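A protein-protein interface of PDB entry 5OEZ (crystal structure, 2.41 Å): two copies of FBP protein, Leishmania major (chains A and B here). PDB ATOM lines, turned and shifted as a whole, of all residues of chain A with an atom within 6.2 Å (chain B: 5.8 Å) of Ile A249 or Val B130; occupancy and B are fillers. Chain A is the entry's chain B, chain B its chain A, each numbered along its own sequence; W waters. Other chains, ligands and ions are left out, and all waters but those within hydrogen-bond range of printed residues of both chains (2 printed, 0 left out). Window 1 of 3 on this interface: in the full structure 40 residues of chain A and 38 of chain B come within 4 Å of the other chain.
Printed residues of chain B that touch a printed residue of chain A: Ala B128, Asn B129, Val B130, Tyr B173, Arg B247, Tyr B248 and Ile B249. Hydrophobic or aromatic side chains of chain B that line the printed part of chain A: Ala B128, Val B130, Tyr B248 and Ile B249. Hydrophobic or aromatic side chains of chain A that line the printed part of chain B: Val A130, Tyr A248 and Ile A249.
Water W1 bridges O of Ile B249 (2.8 Å) and NH1 of Arg A258 (3.1 Å). Water W2 bridges O of Ile A249 (2.9 Å) and NH1 of Arg B258 (3.1 Å).
Val A130 touches Ile B249, and with the chains exchanged Ile A249 touches Val B130. Arg A247 touches Tyr B248, and with the chains exchanged Tyr A248 touches Arg B247. Arg A247 touches Ile B249, and with the chains exchanged Ile A249 touches Arg B247. Tyr A248 touches its own counterpart, Tyr B248. 8 positions are printed for both chains. Of the 12 pairs that touch across the chains among the printed residues, 7 have their exchanged pair printed and touching as well.
Val B130 touches one residue of chain A. Of the printed residues of chain A, Asn B129 touches Ser A131 (3.8 Å) and Ser A175 (3.2 Å). Of the printed residues of chain A, Arg B247 touches Tyr A248, Ile A249 and Gly A250. Printed residues of chain B within 4 Å of Arg A247: Tyr B248 and Ile B249. Printed residues of chain B within 4 Å of Ser A175: Asn B129 (3.2 Å) and Tyr B173 (3.7 Å). Ser B251 touches none of the printed residues of chain A. Ser A251 touches none of the printed residues of chain B. The nearest residue of chain B that does not touch Ile A249 is Tyr B248 (4.1 Å). The nearest printed residue of chain A that does not touch Ile B249 is Tyr A248 (4.04 Å).
Among the printed residues, merely in contact across the chains: Ile A249 with Arg B247 (3.5 Å), Arg A247 with Tyr B248 (3.5 Å), Tyr A248 with Arg B247 (3.5 Å), Arg A247 with Ile B249 (3.5 Å), Ser A175 with Tyr B173 (3.7 Å), Gly A250 with Arg B247 (3.7 Å), Ser A131 with Asn B129 (3.8 Å), Ile A249 with Val B130 (3.9 Å), Val A130 with Ile B249 (3.9 Å) and Arg A258 with Ala B128 (3.9 Å).
The backbone NH (N) of Ser A175 is in hydrogen-bond range of the side-chain amide oxygen (OD1) of Asn B129. The backbone NH (N) of Tyr A248 is in hydrogen-bond range of the backbone carbonyl oxygen (O) of Tyr B248 (2.8 Å).
O of Val B132 lies within hydrogen-bond range of N of Tyr B173, at 2.9 Å. The side-chain hydroxyl of Ser A251 lies close to the backbone carbonyl oxygen of Ser A131, 3.3 Å away. OD1 of Asp A255 is in hydrogen-bond range of N of Ile A249 (2.9 Å). The side-chain carboxylate (OD1) of Asp A255 is in salt-bridge range of the guanidinium group (NH1) of Arg A258, 2.8 Å away. The backbone NH (N) of Val B130 is in hydrogen-bond range of the backbone carbonyl oxygen (O) of Asn B125, at 3.3 Å. The backbone NH (N) of Gly A250 lies within hydrogen-bond range of the side-chain carboxylate (OD2) of Asp A255.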
ATOM      1  N   ASN A 125      26.385 -16.620  32.319  1.00  0.00           N
ATOM      2  CA  ASN A 125      25.467 -17.630  31.772  1.00  0.00           C
ATOM      3  C   ASN A 125      24.377 -18.123  32.724  1.00  0.00           C
ATOM      4  O   ASN A 125      23.366 -18.657  32.258  1.00  0.00           O
ATOM      5  CB  ASN A 125      26.230 -18.880  31.334  1.00  0.00           C
ATOM      6  CG  ASN A 125      27.012 -18.724  30.041  1.00  0.00           C
ATOM      7  OD1 ASN A 125      27.164 -19.706  29.308  1.00  0.00           O
ATOM      8  ND2 ASN A 125      27.550 -17.551  29.766  1.00  0.00           N
ATOM      9  N   VAL A 130      22.250 -21.672  31.357  1.00  0.00           N
ATOM     10  CA  VAL A 130      23.199 -22.436  30.551  1.00  0.00           C
ATOM     11  C   VAL A 130      24.347 -22.957  31.433  1.00  0.00           C
ATOM     12  O   VAL A 130      24.649 -22.354  32.453  1.00  0.00           O
ATOM     13  CB  VAL A 130      23.725 -21.522  29.419  1.00  0.00           C
ATOM     14  CG1 VAL A 130      24.604 -22.291  28.462  1.00  0.00           C
ATOM     15  CG2 VAL A 130      22.556 -20.899  28.665  1.00  0.00           C
ATOM     16  N   SER A 131      24.979 -24.068  31.034  1.00  0.00           N
ATOM     17  CA  SER A 131      26.177 -24.619  31.687  1.00  0.00           C
ATOM     18  C   SER A 131      27.141 -23.568  32.239  1.00  0.00           C
ATOM     19  O   SER A 131      27.481 -22.604  31.551  1.00  0.00           O
ATOM     20  CB  SER A 131      27.003 -25.442  30.670  1.00  0.00           C
ATOM     21  OG  SER A 131      26.418 -26.687  30.319  1.00  0.00           O
ATOM     22  N   SER A 175      22.230 -29.954  33.838  1.00  0.00           N
ATOM     23  CA  SER A 175      21.079 -30.761  34.334  1.00  0.00           C
ATOM     24  C   SER A 175      21.550 -31.907  35.206  1.00  0.00           C
ATOM     25  O   SER A 175      20.862 -32.292  36.133  1.00  0.00           O
ATOM     26  CB  SER A 175      20.186 -31.263  33.189  1.00  0.00           C
ATOM     27  OG  SER A 175      20.944 -31.624  32.048  1.00  0.00           O
ATOM     28  N   SER A 216      33.848 -25.591  17.468  1.00  0.00           N
ATOM     29  CA  SER A 216      33.342 -24.757  18.522  1.00  0.00           C
ATOM     30  C   SER A 216      34.234 -23.515  18.651  1.00  0.00           C
ATOM     31  O   SER A 216      35.381 -23.584  19.119  1.00  0.00           O
ATOM     32  CB  SER A 216      33.306 -25.588  19.827  1.00  0.00           C
ATOM     33  OG  SER A 216      32.506 -24.986  20.835  1.00  0.00           O
ATOM     34  N   ARG A 247      28.821 -25.789  17.211  1.00  0.00           N
ATOM     35  CA  ARG A 247      28.247 -25.657  18.549  1.00  0.00           C
ATOM     36  C   ARG A 247      29.109 -24.702  19.353  1.00  0.00           C
ATOM     37  O   ARG A 247      30.315 -24.895  19.429  1.00  0.00           O
ATOM     38  CB  ARG A 247      28.233 -27.010  19.279  1.00  0.00           C
ATOM     39  CG  ARG A 247      27.339 -28.066  18.644  1.00  0.00           C
ATOM     40  CD  ARG A 247      25.893 -27.693  18.811  1.00  0.00           C
ATOM     41  NE  ARG A 247      24.995 -28.727  18.304  1.00  0.00           N
ATOM     42  CZ  ARG A 247      24.614 -28.878  17.040  1.00  0.00           C
ATOM     43  NH1 ARG A 247      25.055 -28.069  16.069  1.00  0.00           N
ATOM     44  NH2 ARG A 247      23.764 -29.857  16.742  1.00  0.00           N
ATOM     45  N   TYR A 248      28.501 -23.664  19.935  1.00  0.00           N
ATOM     46  CA  TYR A 248      29.199 -22.776  20.860  1.00  0.00           C
ATOM     47  C   TYR A 248      28.244 -22.352  21.968  1.00  0.00           C
ATOM     48  O   TYR A 248      27.445 -21.416  21.826  1.00  0.00           O
ATOM     49  CB  TYR A 248      29.797 -21.567  20.150  1.00  0.00           C
ATOM     50  CG  TYR A 248      30.765 -20.784  21.005  1.00  0.00           C
ATOM     51  CD1 TYR A 248      32.045 -21.281  21.285  1.00  0.00           C
ATOM     52  CD2 TYR A 248      30.435 -19.529  21.499  1.00  0.00           C
ATOM     53  CE1 TYR A 248      32.940 -20.555  22.054  1.00  0.00           C
ATOM     54  CE2 TYR A 248      31.334 -18.804  22.280  1.00  0.00           C
ATOM     55  CZ  TYR A 248      32.580 -19.313  22.546  1.00  0.00           C
ATOM     56  OH  TYR A 248      33.494 -18.599  23.297  1.00  0.00           O
ATOM     57  N   ILE A 249      28.353 -23.068  23.078  1.00  0.00           N
ATOM     58  CA  ILE A 249      27.573 -22.792  24.274  1.00  0.00           C
ATOM     59  C   ILE A 249      27.955 -21.442  24.875  1.00  0.00           C
ATOM     60  O   ILE A 249      27.095 -20.727  25.345  1.00  0.00           O
ATOM     61  CB  ILE A 249      27.764 -23.896  25.334  1.00  0.00           C
ATOM     62  CG1 ILE A 249      27.217 -25.240  24.836  1.00  0.00           C
ATOM     63  CG2 ILE A 249      27.063 -23.524  26.628  1.00  0.00           C
ATOM     64  CD1 ILE A 249      27.756 -26.448  25.604  1.00  0.00           C
ATOM     65  N   GLY A 250      29.239 -21.085  24.837  1.00  0.00           N
ATOM     66  CA  GLY A 250      29.720 -19.866  25.510  1.00  0.00           C
ATOM     67  C   GLY A 250      30.133 -20.087  26.956  1.00  0.00           C
ATOM     68  O   GLY A 250      30.305 -19.131  27.713  1.00  0.00           O
ATOM     69  N   SER A 251      30.281 -21.349  27.334  1.00  0.00           N
ATOM     70  CA  SER A 251      30.895 -21.733  28.584  1.00  0.00           C
ATOM     71  C   SER A 251      32.035 -22.667  28.206  1.00  0.00           C
ATOM     72  O   SER A 251      31.801 -23.737  27.639  1.00  0.00           O
ATOM     73  CB  SER A 251      29.869 -22.434  29.471  1.00  0.00           C
ATOM     74  OG  SER A 251      30.493 -23.260  30.451  1.00  0.00           O
ATOM     75  N   GLY A 254      31.675 -26.252  29.524  1.00  0.00           N
ATOM     76  CA  GLY A 254      30.637 -26.940  28.753  1.00  0.00           C
ATOM     77  C   GLY A 254      31.097 -27.336  27.362  1.00  0.00           C
ATOM     78  O   GLY A 254      30.889 -28.469  26.932  1.00  0.00           O
ATOM     79  N   ASP A 255      31.774 -26.427  26.662  1.00  0.00           N
ATOM     80  CA  ASP A 255      32.214 -26.720  25.291  1.00  0.00           C
ATOM     81  C   ASP A 255      33.328 -27.765  25.265  1.00  0.00           C
ATOM     82  O   ASP A 255      33.301 -28.696  24.445  1.00  0.00           O
ATOM     83  CB  ASP A 255      32.600 -25.437  24.541  1.00  0.00           C
ATOM     84  CG  ASP A 255      31.354 -24.581  24.126  1.00  0.00           C
ATOM     85  OD1 ASP A 255      30.444 -25.117  23.432  1.00  0.00           O
ATOM     86  OD2 ASP A 255      31.309 -23.363  24.456  1.00  0.00           O
ATOM     87  N   ARG A 258      31.750 -31.301  26.082  1.00  0.00           N
ATOM     88  CA  ARG A 258      31.178 -31.885  24.850  1.00  0.00           C
ATOM     89  C   ARG A 258      32.298 -32.394  23.928  1.00  0.00           C
ATOM     90  O   ARG A 258      32.195 -33.471  23.359  1.00  0.00           O
ATOM     91  CB  ARG A 258      30.306 -30.852  24.111  1.00  0.00           C
ATOM     92  CG  ARG A 258      29.490 -31.418  22.943  1.00  0.00           C
ATOM     93  CD  ARG A 258      28.980 -30.351  21.970  1.00  0.00           C
ATOM     94  NE  ARG A 258      30.090 -29.506  21.553  1.00  0.00           N
ATOM     95  CZ  ARG A 258      30.288 -28.231  21.899  1.00  0.00           C
ATOM     96  NH1 ARG A 258      29.403 -27.534  22.622  1.00  0.00           N
ATOM     97  NH2 ARG A 258      31.399 -27.638  21.498  1.00  0.00           N
ATOM     98  N   ASN B 125      21.780 -34.278  23.157  1.00  0.00           N
ATOM     99  CA  ASN B 125      22.550 -33.411  24.064  1.00  0.00           C
ATOM    100  C   ASN B 125      22.722 -33.897  25.493  1.00  0.00           C
ATOM    101  O   ASN B 125      23.650 -33.453  26.170  1.00  0.00           O
ATOM    102  CB  ASN B 125      21.891 -32.038  24.175  1.00  0.00           C
ATOM    103  CG  ASN B 125      22.052 -31.199  22.931  1.00  0.00           C
ATOM    104  OD1 ASN B 125      22.890 -31.467  22.083  1.00  0.00           O
ATOM    105  ND2 ASN B 125      21.239 -30.167  22.821  1.00  0.00           N
ATOM    106  N   ILE B 126      21.844 -34.788  25.953  1.00  0.00           N
ATOM    107  CA  ILE B 126      21.880 -35.308  27.327  1.00  0.00           C
ATOM    108  C   ILE B 126      23.255 -35.890  27.661  1.00  0.00           C
ATOM    109  O   ILE B 126      23.754 -35.695  28.771  1.00  0.00           O
ATOM    110  CB  ILE B 126      20.764 -36.372  27.641  1.00  0.00           C
ATOM    111  CG1 ILE B 126      20.987 -37.610  26.691  1.00  0.00           C
ATOM    112  CG2 ILE B 126      19.351 -35.747  27.662  1.00  0.00           C
ATOM    113  CD1 ILE B 126      19.864 -38.589  26.386  1.00  0.00           C
ATOM    114  N   ALA B 128      26.263 -35.102  26.784  1.00  0.00           N
ATOM    115  CA  ALA B 128      27.230 -34.047  27.073  1.00  0.00           C
ATOM    116  C   ALA B 128      26.728 -33.048  28.109  1.00  0.00           C
ATOM    117  O   ALA B 128      27.339 -31.988  28.275  1.00  0.00           O
ATOM    118  CB  ALA B 128      27.580 -33.311  25.792  1.00  0.00           C
ATOM    119  N   ASN B 129      25.611 -33.354  28.784  1.00  0.00           N
ATOM    120  CA  ASN B 129      25.090 -32.513  29.873  1.00  0.00           C
ATOM    121  C   ASN B 129      24.732 -31.083  29.463  1.00  0.00           C
ATOM    122  O   ASN B 129      24.908 -30.139  30.224  1.00  0.00           O
ATOM    123  CB  ASN B 129      26.108 -32.495  31.034  1.00  0.00           C
ATOM    124  CG  ASN B 129      25.491 -32.081  32.359  1.00  0.00           C
ATOM    125  OD1 ASN B 129      24.266 -32.017  32.502  1.00  0.00           O
ATOM    126  ND2 ASN B 129      26.347 -31.797  33.344  1.00  0.00           N
ATOM    127  N   VAL B 130      24.267 -30.918  28.245  1.00  0.00           N
ATOM    128  CA  VAL B 130      23.805 -29.624  27.760  1.00  0.00           C
ATOM    129  C   VAL B 130      22.274 -29.543  27.876  1.00  0.00           C
ATOM    130  O   VAL B 130      21.612 -30.566  27.859  1.00  0.00           O
ATOM    131  CB  VAL B 130      24.272 -29.459  26.299  1.00  0.00           C
ATOM    132  CG1 VAL B 130      23.937 -28.076  25.777  1.00  0.00           C
ATOM    133  CG2 VAL B 130      25.770 -29.708  26.202  1.00  0.00           C
ATOM    134  N   SER B 131      21.728 -28.334  28.026  1.00  0.00           N
ATOM    135  CA  SER B 131      20.285 -28.069  28.037  1.00  0.00           C
ATOM    136  C   SER B 131      19.479 -28.955  27.089  1.00  0.00           C
ATOM    137  O   SER B 131      19.850 -29.151  25.930  1.00  0.00           O
ATOM    138  CB  SER B 131      20.013 -26.624  27.553  1.00  0.00           C
ATOM    139  OG  SER B 131      20.353 -25.626  28.497  1.00  0.00           O
ATOM    140  N   VAL B 132      18.365 -29.457  27.591  1.00  0.00           N
ATOM    141  CA  VAL B 132      17.298 -29.989  26.753  1.00  0.00           C
ATOM    142  C   VAL B 132      15.986 -29.344  27.194  1.00  0.00           C
ATOM    143  O   VAL B 132      15.974 -28.545  28.125  1.00  0.00           O
ATOM    144  CB  VAL B 132      17.226 -31.521  26.812  1.00  0.00           C
ATOM    145  CG1 VAL B 132      18.489 -32.116  26.243  1.00  0.00           C
ATOM    146  CG2 VAL B 132      17.016 -32.011  28.226  1.00  0.00           C
ATOM    147  N   TYR B 173      15.455 -27.872  30.945  1.00  0.00           N
ATOM    148  CA  TYR B 173      16.120 -28.701  31.924  1.00  0.00           C
ATOM    149  C   TYR B 173      17.606 -28.367  31.838  1.00  0.00           C
ATOM    150  O   TYR B 173      18.331 -28.885  30.996  1.00  0.00           O
ATOM    151  CB  TYR B 173      15.862 -30.173  31.629  1.00  0.00           C
ATOM    152  CG  TYR B 173      14.397 -30.516  31.426  1.00  0.00           C
ATOM    153  CD1 TYR B 173      13.562 -30.752  32.495  1.00  0.00           C
ATOM    154  CD2 TYR B 173      13.853 -30.605  30.145  1.00  0.00           C
ATOM    155  CE1 TYR B 173      12.223 -31.082  32.307  1.00  0.00           C
ATOM    156  CE2 TYR B 173      12.520 -30.919  29.943  1.00  0.00           C
ATOM    157  CZ  TYR B 173      11.705 -31.157  31.030  1.00  0.00           C
ATOM    158  OH  TYR B 173      10.387 -31.502  30.826  1.00  0.00           O
ATOM    159  N   ARG B 247      26.177 -17.342  19.823  1.00  0.00           N
ATOM    160  CA  ARG B 247      25.878 -18.427  20.767  1.00  0.00           C
ATOM    161  C   ARG B 247      24.961 -19.431  20.075  1.00  0.00           C
ATOM    162  O   ARG B 247      23.952 -19.036  19.525  1.00  0.00           O
ATOM    163  CB  ARG B 247      25.136 -17.905  22.005  1.00  0.00           C
ATOM    164  CG  ARG B 247      25.928 -16.956  22.889  1.00  0.00           C
ATOM    165  CD  ARG B 247      27.071 -17.690  23.557  1.00  0.00           C
ATOM    166  NE  ARG B 247      27.791 -16.840  24.483  1.00  0.00           N
ATOM    167  CZ  ARG B 247      28.781 -16.014  24.159  1.00  0.00           C
ATOM    168  NH1 ARG B 247      29.195 -15.854  22.896  1.00  0.00           N
ATOM    169  NH2 ARG B 247      29.364 -15.316  25.124  1.00  0.00           N
ATOM    170  N   TYR B 248      25.360 -20.695  20.029  1.00  0.00           N
ATOM    171  CA  TYR B 248      24.510 -21.760  19.511  1.00  0.00           C
ATOM    172  C   TYR B 248      24.726 -23.027  20.333  1.00  0.00           C
ATOM    173  O   TYR B 248      25.681 -23.801  20.112  1.00  0.00           O
ATOM    174  CB  TYR B 248      24.745 -22.029  18.030  1.00  0.00           C
ATOM    175  CG  TYR B 248      23.690 -22.906  17.388  1.00  0.00           C
ATOM    176  CD1 TYR B 248      22.408 -22.415  17.130  1.00  0.00           C
ATOM    177  CD2 TYR B 248      23.975 -24.204  17.008  1.00  0.00           C
ATOM    178  CE1 TYR B 248      21.447 -23.189  16.496  1.00  0.00           C
ATOM    179  CE2 TYR B 248      23.007 -25.002  16.403  1.00  0.00           C
ATOM    180  CZ  TYR B 248      21.749 -24.479  16.144  1.00  0.00           C
ATOM    181  OH  TYR B 248      20.811 -25.257  15.527  1.00  0.00           O
ATOM    182  N   ILE B 249      23.850 -23.183  21.319  1.00  0.00           N
ATOM    183  CA  ILE B 249      23.852 -24.339  22.202  1.00  0.00           C
ATOM    184  C   ILE B 249      23.549 -25.612  21.421  1.00  0.00           C
ATOM    185  O   ILE B 249      24.131 -26.642  21.698  1.00  0.00           O
ATOM    186  CB  ILE B 249      22.836 -24.172  23.349  1.00  0.00           C
ATOM    187  CG1 ILE B 249      23.215 -23.015  24.273  1.00  0.00           C
ATOM    188  CG2 ILE B 249      22.752 -25.437  24.186  1.00  0.00           C
ATOM    189  CD1 ILE B 249      22.058 -22.500  25.127  1.00  0.00           C
ATOM    190  N   SER B 251      20.348 -26.690  21.266  1.00  0.00           N
ATOM    191  CA  SER B 251      19.086 -27.089  21.821  1.00  0.00           C
ATOM    192  C   SER B 251      18.196 -25.892  21.579  1.00  0.00           C
ATOM    193  O   SER B 251      18.420 -24.809  22.139  1.00  0.00           O
ATOM    194  CB  SER B 251      19.212 -27.394  23.331  1.00  0.00           C
ATOM    195  OG  SER B 251      17.970 -27.277  24.032  1.00  0.00           O
ATOM    196  N   ARG B 258      17.412 -18.342  26.216  1.00  0.00           N
ATOM    197  CA  ARG B 258      18.429 -17.278  26.284  1.00  0.00           C
ATOM    198  C   ARG B 258      17.975 -16.044  25.487  1.00  0.00           C
ATOM    199  O   ARG B 258      18.074 -14.918  25.972  1.00  0.00           O
ATOM    200  CB  ARG B 258      19.791 -17.760  25.747  1.00  0.00           C
ATOM    201  CG  ARG B 258      20.956 -16.772  26.000  1.00  0.00           C
ATOM    202  CD  ARG B 258      22.176 -17.035  25.119  1.00  0.00           C
ATOM    203  NE  ARG B 258      21.747 -17.118  23.726  1.00  0.00           N
ATOM    204  CZ  ARG B 258      21.709 -18.215  22.970  1.00  0.00           C
ATOM    205  NH1 ARG B 258      22.175 -19.398  23.400  1.00  0.00           N
ATOM    206  NH2 ARG B 258      21.225 -18.118  21.731  1.00  0.00           N
HETATM  207  O   HOH W   1      26.412 -28.120  22.426  1.00  0.00           O
HETATM  208  O   HOH W   2      24.561 -19.393  25.389  1.00  0.00           O
